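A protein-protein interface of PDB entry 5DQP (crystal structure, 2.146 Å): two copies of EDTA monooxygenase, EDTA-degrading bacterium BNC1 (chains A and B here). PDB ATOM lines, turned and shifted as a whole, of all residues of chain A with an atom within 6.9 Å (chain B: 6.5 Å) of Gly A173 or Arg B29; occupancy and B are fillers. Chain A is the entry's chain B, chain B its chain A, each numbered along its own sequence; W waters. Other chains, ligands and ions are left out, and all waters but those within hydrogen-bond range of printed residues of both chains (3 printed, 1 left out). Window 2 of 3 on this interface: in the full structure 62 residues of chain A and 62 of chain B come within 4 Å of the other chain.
Of the printed residues of chain B, Ala A171 touches Gly B27, Asn B28, Arg B29 and Ala B30. Of the printed residues of chain B, Ile A172 touches Gly B27 (3.8 Å), Asn B28 (3.6 Å) and Arg B29 (3.7 Å). Pro A174 touches none of the printed residues of chain B. Asn A177 touches none of the printed residues of chain B. Arg B29 touches just these residues of chain A: Glu A170, Ala A171, Ile A172, Gly A173, Asn A175 and Pro A178. Of the printed residues of chain A, Ala B30 touches Ala A171 (3.8 Å). The nearest residue of chain B that does not touch Gly A173 is Gly B27 (4.3 Å). The nearest residue of chain A that does not touch Arg B29 is Phe A166 (4.4 Å). The nearest printed residue of chain A that does not touch Gly B27 is Gly A173 (4.3 Å).
No position is printed for both chains. Of the 14 pairs that touch across the chains among the printed residues, none has its exchanged pair printed and touching as well.
Among the printed residues, pairs that only touch across the chains: Phe A166 with Phe B33 (3.9 Å), Ala A171 with Gly B27 (3.8 Å), Ala A171 with Asn B28 (3.8 Å), Ala A171 with Ala B30 (3.8 Å), Ile A172 with Gly B27 (3.8 Å), Ile A172 with Asn B28 (3.6 Å), Ile A172 with Arg B29 (3.7 Å), Asn A175 with Arg B29 (3.4 Å), Pro A178 with Trp B22 (3.8 Å), Pro A178 with Arg B29 (3.8 Å) and Phe A179 with Trp B22 (3.96 Å).
O of Glu A170 sits at hydrogen-bond distance from NH2 of Arg B29, at 3.0 Å. NH1 of Arg B29 is in hydrogen-bond range of O of Gly A173 (2.8 Å). The backbone NH (N) of Arg B29 sits at hydrogen-bond distance from the backbone carbonyl oxygen (O) of Ala A171 (2.8 Å).
The side-chain amide oxygen (OD1) of Asn B23 is in hydrogen-bond range of the guanidinium group (NH1) of Arg B29, at 2.6 Å. ND2 of Asn A175 sits at hydrogen-bond distance from O of Glu A170. O of Trp B22 lies within hydrogen-bond range of NH1 of Arg B31, at 3.0 Å. The side-chain amide oxygen of Asn B28 lies close to the backbone NH of Ala B30 (3.1 Å). The backbone carbonyl oxygen (O) of Asn B28 sits close to the guanidinium group (NH1) of Arg B31, at 3.2 Å. The backbone NH (N) of Asn A177 sits at hydrogen-bond distance from the side-chain amide oxygen (OD1) of Asn A175 (3.0 Å).
Printed residues of chain A that touch a printed residue of chain B: Phe A166, Glu A170, Ala A171, Ile A172, Gly A173, Asn A175, Pro A178 and Phe A179. Of the 10 printed residues of chain B, 6 touch a printed residue of chain A. Printed residues of chain B that touch a printed residue of chain A: Trp B22, Gly B27, Asn B28, Arg B29, Ala B30 and Phe B33. Along chain B the printed residues that touch a printed residue of chain A span positions 22 to 33. Among the printed residues, 14 pairs touch across the chains.
Water W2 lies within hydrogen-bond range of O of Gly B27, OD1 of Asn B23 and N of Gly A173. Water W1 lies within hydrogen-bond range of the backbone carbonyl oxygen of Pro A178, the guanidinium group of Arg B29 and the backbone carbonyl oxygen of Glu A170. Water W3 lies within hydrogen-bond range of OD1 of Asn B23 (3.4 Å) and O of Gly A173 (3.5 Å).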
ATOM      1  N   PHE A 166     -35.302  -4.782 -10.480  1.00  0.00           N
ATOM      2  CA  PHE A 166     -34.222  -5.653 -10.064  1.00  0.00           C
ATOM      3  C   PHE A 166     -32.937  -5.298 -10.811  1.00  0.00           C
ATOM      4  O   PHE A 166     -32.981  -5.028 -12.011  1.00  0.00           O
ATOM      5  CB  PHE A 166     -34.619  -7.099 -10.363  1.00  0.00           C
ATOM      6  CG  PHE A 166     -33.602  -8.124  -9.936  1.00  0.00           C
ATOM      7  CD1 PHE A 166     -33.477  -8.471  -8.604  1.00  0.00           C
ATOM      8  CD2 PHE A 166     -32.801  -8.749 -10.859  1.00  0.00           C
ATOM      9  CE1 PHE A 166     -32.554  -9.423  -8.195  1.00  0.00           C
ATOM     10  CE2 PHE A 166     -31.886  -9.708 -10.452  1.00  0.00           C
ATOM     11  CZ  PHE A 166     -31.761 -10.033  -9.106  1.00  0.00           C
ATOM     12  N   PRO A 167     -31.762  -5.333 -10.145  1.00  0.00           N
ATOM     13  CA  PRO A 167     -30.513  -4.944 -10.828  1.00  0.00           C
ATOM     14  C   PRO A 167     -29.904  -6.070 -11.659  1.00  0.00           C
ATOM     15  O   PRO A 167     -29.013  -6.796 -11.195  1.00  0.00           O
ATOM     16  CB  PRO A 167     -29.601  -4.536  -9.664  1.00  0.00           C
ATOM     17  CG  PRO A 167     -30.059  -5.437  -8.522  1.00  0.00           C
ATOM     18  CD  PRO A 167     -31.532  -5.758  -8.753  1.00  0.00           C
ATOM     19  N   GLU A 170     -26.203  -6.522 -11.624  1.00  0.00           N
ATOM     20  CA  GLU A 170     -25.497  -6.820 -10.398  1.00  0.00           C
ATOM     21  C   GLU A 170     -26.242  -7.878  -9.582  1.00  0.00           C
ATOM     22  O   GLU A 170     -26.655  -7.644  -8.487  1.00  0.00           O
ATOM     23  CB  GLU A 170     -25.315  -5.558  -9.563  1.00  0.00           C
ATOM     24  CG  GLU A 170     -25.283  -4.240 -10.299  1.00  0.00           C
ATOM     25  CD  GLU A 170     -25.228  -3.071  -9.350  1.00  0.00           C
ATOM     26  OE1 GLU A 170     -26.065  -2.179  -9.437  1.00  0.00           O
ATOM     27  OE2 GLU A 170     -24.351  -3.030  -8.494  1.00  0.00           O
ATOM     28  N   ALA A 171     -26.382  -9.042 -10.179  1.00  0.00           N
ATOM     29  CA  ALA A 171     -27.085 -10.161  -9.572  1.00  0.00           C
ATOM     30  C   ALA A 171     -26.140 -11.263  -9.098  1.00  0.00           C
ATOM     31  O   ALA A 171     -26.611 -12.280  -8.592  1.00  0.00           O
ATOM     32  CB  ALA A 171     -28.113 -10.734 -10.554  1.00  0.00           C
ATOM     33  N   ILE A 172     -24.829 -11.086  -9.238  1.00  0.00           N
ATOM     34  CA  ILE A 172     -23.841 -12.090  -8.851  1.00  0.00           C
ATOM     35  C   ILE A 172     -22.839 -11.429  -7.916  1.00  0.00           C
ATOM     36  O   ILE A 172     -22.182 -10.460  -8.301  1.00  0.00           O
ATOM     37  CB  ILE A 172     -23.125 -12.701 -10.073  1.00  0.00           C
ATOM     38  CG1 ILE A 172     -24.113 -13.499 -10.938  1.00  0.00           C
ATOM     39  CG2 ILE A 172     -21.999 -13.625  -9.623  1.00  0.00           C
ATOM     40  CD1 ILE A 172     -23.571 -13.909 -12.314  1.00  0.00           C
ATOM     41  N   GLY A 173     -22.745 -11.930  -6.683  1.00  0.00           N
ATOM     42  CA  GLY A 173     -21.716 -11.517  -5.766  1.00  0.00           C
ATOM     43  C   GLY A 173     -22.149 -10.378  -4.863  1.00  0.00           C
ATOM     44  O   GLY A 173     -23.321  -9.977  -4.849  1.00  0.00           O
ATOM     45  N   PRO A 174     -21.196  -9.820  -4.112  1.00  0.00           N
ATOM     46  CA  PRO A 174     -21.543  -8.832  -3.072  1.00  0.00           C
ATOM     47  C   PRO A 174     -22.387  -7.694  -3.623  1.00  0.00           C
ATOM     48  O   PRO A 174     -22.112  -7.128  -4.686  1.00  0.00           O
ATOM     49  CB  PRO A 174     -20.176  -8.348  -2.566  1.00  0.00           C
ATOM     50  CG  PRO A 174     -19.268  -9.582  -2.780  1.00  0.00           C
ATOM     51  CD  PRO A 174     -19.752 -10.139  -4.123  1.00  0.00           C
ATOM     52  N   ASN A 175     -23.510  -7.453  -2.994  1.00  0.00           N
ATOM     53  CA  ASN A 175     -24.372  -6.334  -3.279  1.00  0.00           C
ATOM     54  C   ASN A 175     -25.151  -6.100  -2.024  1.00  0.00           C
ATOM     55  O   ASN A 175     -25.892  -6.948  -1.644  1.00  0.00           O
ATOM     56  CB  ASN A 175     -25.305  -6.673  -4.442  1.00  0.00           C
ATOM     57  CG  ASN A 175     -26.007  -5.457  -5.031  1.00  0.00           C
ATOM     58  OD1 ASN A 175     -26.079  -4.415  -4.438  1.00  0.00           O
ATOM     59  ND2 ASN A 175     -26.537  -5.618  -6.210  1.00  0.00           N
ATOM     60  N   PRO A 176     -25.036  -4.940  -1.404  1.00  0.00           N
ATOM     61  CA  PRO A 176     -25.874  -4.632  -0.232  1.00  0.00           C
ATOM     62  C   PRO A 176     -27.313  -4.303  -0.591  1.00  0.00           C
ATOM     63  O   PRO A 176     -28.147  -4.182   0.315  1.00  0.00           O
ATOM     64  CB  PRO A 176     -25.176  -3.415   0.373  1.00  0.00           C
ATOM     65  CG  PRO A 176     -24.662  -2.698  -0.822  1.00  0.00           C
ATOM     66  CD  PRO A 176     -24.225  -3.782  -1.814  1.00  0.00           C
ATOM     67  N   ASN A 177     -27.621  -4.135  -1.877  1.00  0.00           N
ATOM     68  CA  ASN A 177     -28.968  -3.807  -2.339  1.00  0.00           C
ATOM     69  C   ASN A 177     -29.399  -4.797  -3.420  1.00  0.00           C
ATOM     70  O   ASN A 177     -29.583  -4.425  -4.580  1.00  0.00           O
ATOM     71  CB  ASN A 177     -28.993  -2.374  -2.860  1.00  0.00           C
ATOM     72  CG  ASN A 177     -30.374  -1.941  -3.304  1.00  0.00           C
ATOM     73  OD1 ASN A 177     -31.370  -2.512  -2.864  1.00  0.00           O
ATOM     74  ND2 ASN A 177     -30.442  -0.906  -4.154  1.00  0.00           N
ATOM     75  N   PRO A 178     -29.544  -6.081  -3.080  1.00  0.00           N
ATOM     76  CA  PRO A 178     -29.819  -7.081  -4.126  1.00  0.00           C
ATOM     77  C   PRO A 178     -31.185  -6.946  -4.781  1.00  0.00           C
ATOM     78  O   PRO A 178     -31.352  -7.429  -5.909  1.00  0.00           O
ATOM     79  CB  PRO A 178     -29.689  -8.420  -3.384  1.00  0.00           C
ATOM     80  CG  PRO A 178     -29.880  -8.050  -1.898  1.00  0.00           C
ATOM     81  CD  PRO A 178     -29.198  -6.713  -1.796  1.00  0.00           C
ATOM     82  N   PHE A 179     -32.169  -6.319  -4.130  1.00  0.00           N
ATOM     83  CA  PHE A 179     -33.469  -6.165  -4.769  1.00  0.00           C
ATOM     84  C   PHE A 179     -33.539  -4.999  -5.744  1.00  0.00           C
ATOM     85  O   PHE A 179     -34.489  -4.950  -6.544  1.00  0.00           O
ATOM     86  CB  PHE A 179     -34.573  -5.979  -3.732  1.00  0.00           C
ATOM     87  CG  PHE A 179     -35.024  -7.242  -3.120  1.00  0.00           C
ATOM     88  CD1 PHE A 179     -34.303  -7.818  -2.093  1.00  0.00           C
ATOM     89  CD2 PHE A 179     -36.179  -7.871  -3.573  1.00  0.00           C
ATOM     90  CE1 PHE A 179     -34.728  -9.026  -1.522  1.00  0.00           C
ATOM     91  CE2 PHE A 179     -36.590  -9.065  -3.017  1.00  0.00           C
ATOM     92  CZ  PHE A 179     -35.856  -9.636  -1.982  1.00  0.00           C
ATOM     93  N   SER B  15     -35.152 -20.050  -5.022  1.00  0.00           N
ATOM     94  CA  SER B  15     -33.806 -20.609  -4.998  1.00  0.00           C
ATOM     95  C   SER B  15     -33.622 -21.660  -3.918  1.00  0.00           C
ATOM     96  O   SER B  15     -32.525 -22.202  -3.777  1.00  0.00           O
ATOM     97  CB  SER B  15     -32.776 -19.489  -4.802  1.00  0.00           C
ATOM     98  OG  SER B  15     -33.083 -18.724  -3.649  1.00  0.00           O
ATOM     99  N   TRP B  22     -30.254 -17.863  -2.722  1.00  0.00           N
ATOM    100  CA  TRP B  22     -29.992 -17.385  -4.073  1.00  0.00           C
ATOM    101  C   TRP B  22     -28.555 -16.938  -4.285  1.00  0.00           C
ATOM    102  O   TRP B  22     -28.171 -16.684  -5.433  1.00  0.00           O
ATOM    103  CB  TRP B  22     -30.939 -16.256  -4.456  1.00  0.00           C
ATOM    104  CG  TRP B  22     -30.908 -15.034  -3.608  1.00  0.00           C
ATOM    105  CD1 TRP B  22     -30.329 -14.883  -2.368  1.00  0.00           C
ATOM    106  CD2 TRP B  22     -31.500 -13.763  -3.932  1.00  0.00           C
ATOM    107  NE1 TRP B  22     -30.554 -13.610  -1.907  1.00  0.00           N
ATOM    108  CE2 TRP B  22     -31.252 -12.897  -2.848  1.00  0.00           C
ATOM    109  CE3 TRP B  22     -32.205 -13.271  -5.045  1.00  0.00           C
ATOM    110  CZ2 TRP B  22     -31.690 -11.561  -2.836  1.00  0.00           C
ATOM    111  CZ3 TRP B  22     -32.639 -11.937  -5.032  1.00  0.00           C
ATOM    112  CH2 TRP B  22     -32.391 -11.112  -3.937  1.00  0.00           C
ATOM    113  N   ASN B  23     -27.766 -16.809  -3.222  1.00  0.00           N
ATOM    114  CA  ASN B  23     -26.335 -16.580  -3.317  1.00  0.00           C
ATOM    115  C   ASN B  23     -25.512 -17.876  -3.230  1.00  0.00           C
ATOM    116  O   ASN B  23     -24.284 -17.809  -3.270  1.00  0.00           O
ATOM    117  CB  ASN B  23     -25.885 -15.602  -2.218  1.00  0.00           C
ATOM    118  CG  ASN B  23     -26.234 -14.156  -2.539  1.00  0.00           C
ATOM    119  OD1 ASN B  23     -25.981 -13.667  -3.652  1.00  0.00           O
ATOM    120  ND2 ASN B  23     -26.824 -13.461  -1.563  1.00  0.00           N
ATOM    121  N   GLY B  27     -24.461 -19.158  -7.478  1.00  0.00           N
ATOM    122  CA  GLY B  27     -24.501 -17.807  -6.948  1.00  0.00           C
ATOM    123  C   GLY B  27     -25.097 -16.737  -7.838  1.00  0.00           C
ATOM    124  O   GLY B  27     -24.864 -15.553  -7.590  1.00  0.00           O
ATOM    125  N   ASN B  28     -25.855 -17.107  -8.874  1.00  0.00           N
ATOM    126  CA  ASN B  28     -26.484 -16.128  -9.765  1.00  0.00           C
ATOM    127  C   ASN B  28     -27.881 -15.822  -9.238  1.00  0.00           C
ATOM    128  O   ASN B  28     -28.829 -16.576  -9.458  1.00  0.00           O
ATOM    129  CB  ASN B  28     -26.514 -16.644 -11.207  1.00  0.00           C
ATOM    130  CG  ASN B  28     -27.170 -15.654 -12.183  1.00  0.00           C
ATOM    131  OD1 ASN B  28     -27.502 -14.519 -11.817  1.00  0.00           O
ATOM    132  ND2 ASN B  28     -27.363 -16.090 -13.424  1.00  0.00           N
ATOM    133  N   ARG B  29     -28.032 -14.694  -8.555  1.00  0.00           N
ATOM    134  CA  ARG B  29     -29.330 -14.406  -7.963  1.00  0.00           C
ATOM    135  C   ARG B  29     -30.434 -14.341  -9.013  1.00  0.00           C
ATOM    136  O   ARG B  29     -31.601 -14.609  -8.701  1.00  0.00           O
ATOM    137  CB  ARG B  29     -29.256 -13.106  -7.157  1.00  0.00           C
ATOM    138  CG  ARG B  29     -28.459 -13.269  -5.838  1.00  0.00           C
ATOM    139  CD  ARG B  29     -28.486 -11.977  -4.988  1.00  0.00           C
ATOM    140  NE  ARG B  29     -27.837 -10.823  -5.623  1.00  0.00           N
ATOM    141  CZ  ARG B  29     -26.529 -10.556  -5.546  1.00  0.00           C
ATOM    142  NH1 ARG B  29     -25.721 -11.358  -4.882  1.00  0.00           N
ATOM    143  NH2 ARG B  29     -26.028  -9.497  -6.160  1.00  0.00           N
ATOM    144  N   ALA B  30     -30.098 -13.966 -10.248  1.00  0.00           N
ATOM    145  CA  ALA B  30     -31.110 -13.788 -11.286  1.00  0.00           C
ATOM    146  C   ALA B  30     -31.682 -15.109 -11.814  1.00  0.00           C
ATOM    147  O   ALA B  30     -32.605 -15.070 -12.639  1.00  0.00           O
ATOM    148  CB  ALA B  30     -30.518 -12.979 -12.451  1.00  0.00           C
ATOM    149  N   ARG B  31     -31.177 -16.273 -11.382  1.00  0.00           N
ATOM    150  CA  ARG B  31     -31.733 -17.528 -11.884  1.00  0.00           C
ATOM    151  C   ARG B  31     -33.140 -17.792 -11.373  1.00  0.00           C
ATOM    152  O   ARG B  31     -33.837 -18.623 -11.960  1.00  0.00           O
ATOM    153  CB  ARG B  31     -30.836 -18.709 -11.505  1.00  0.00           C
ATOM    154  CG  ARG B  31     -30.743 -18.903 -10.015  1.00  0.00           C
ATOM    155  CD  ARG B  31     -29.766 -19.995  -9.682  1.00  0.00           C
ATOM    156  NE  ARG B  31     -30.013 -20.529  -8.353  1.00  0.00           N
ATOM    157  CZ  ARG B  31     -29.449 -20.054  -7.253  1.00  0.00           C
ATOM    158  NH1 ARG B  31     -28.603 -19.018  -7.331  1.00  0.00           N
ATOM    159  NH2 ARG B  31     -29.727 -20.625  -6.083  1.00  0.00           N
ATOM    160  N   ILE B  32     -33.582 -17.129 -10.297  1.00  0.00           N
ATOM    161  CA  ILE B  32     -34.959 -17.350  -9.859  1.00  0.00           C
ATOM    162  C   ILE B  32     -35.970 -16.726 -10.807  1.00  0.00           C
ATOM    163  O   ILE B  32     -37.181 -16.948 -10.653  1.00  0.00           O
ATOM    164  CB  ILE B  32     -35.213 -16.841  -8.421  1.00  0.00           C
ATOM    165  CG1 ILE B  32     -35.118 -15.319  -8.344  1.00  0.00           C
ATOM    166  CG2 ILE B  32     -34.219 -17.490  -7.452  1.00  0.00           C
ATOM    167  CD1 ILE B  32     -35.469 -14.775  -6.955  1.00  0.00           C
ATOM    168  N   PHE B  33     -35.514 -15.949 -11.782  1.00  0.00           N
ATOM    169  CA  PHE B  33     -36.389 -15.378 -12.791  1.00  0.00           C
ATOM    170  C   PHE B  33     -36.283 -16.089 -14.133  1.00  0.00           C
ATOM    171  O   PHE B  33     -36.784 -15.578 -15.139  1.00  0.00           O
ATOM    172  CB  PHE B  33     -36.085 -13.888 -12.942  1.00  0.00           C
ATOM    173  CG  PHE B  33     -36.176 -13.122 -11.639  1.00  0.00           C
ATOM    174  CD1 PHE B  33     -37.398 -12.985 -10.988  1.00  0.00           C
ATOM    175  CD2 PHE B  33     -35.037 -12.564 -11.064  1.00  0.00           C
ATOM    176  CE1 PHE B  33     -37.492 -12.293  -9.798  1.00  0.00           C
ATOM    177  CE2 PHE B  33     -35.117 -11.872  -9.867  1.00  0.00           C
ATOM    178  CZ  PHE B  33     -36.351 -11.736  -9.235  1.00  0.00           C
HETATM  179  O   HOH W   1     -29.196  -8.762  -7.131  1.00  0.00           O
HETATM  180  O   HOH W   2     -23.939 -14.446  -5.423  1.00  0.00           O
HETATM  181  O   HOH W   3     -23.823 -11.723  -1.886  1.00  0.00           O
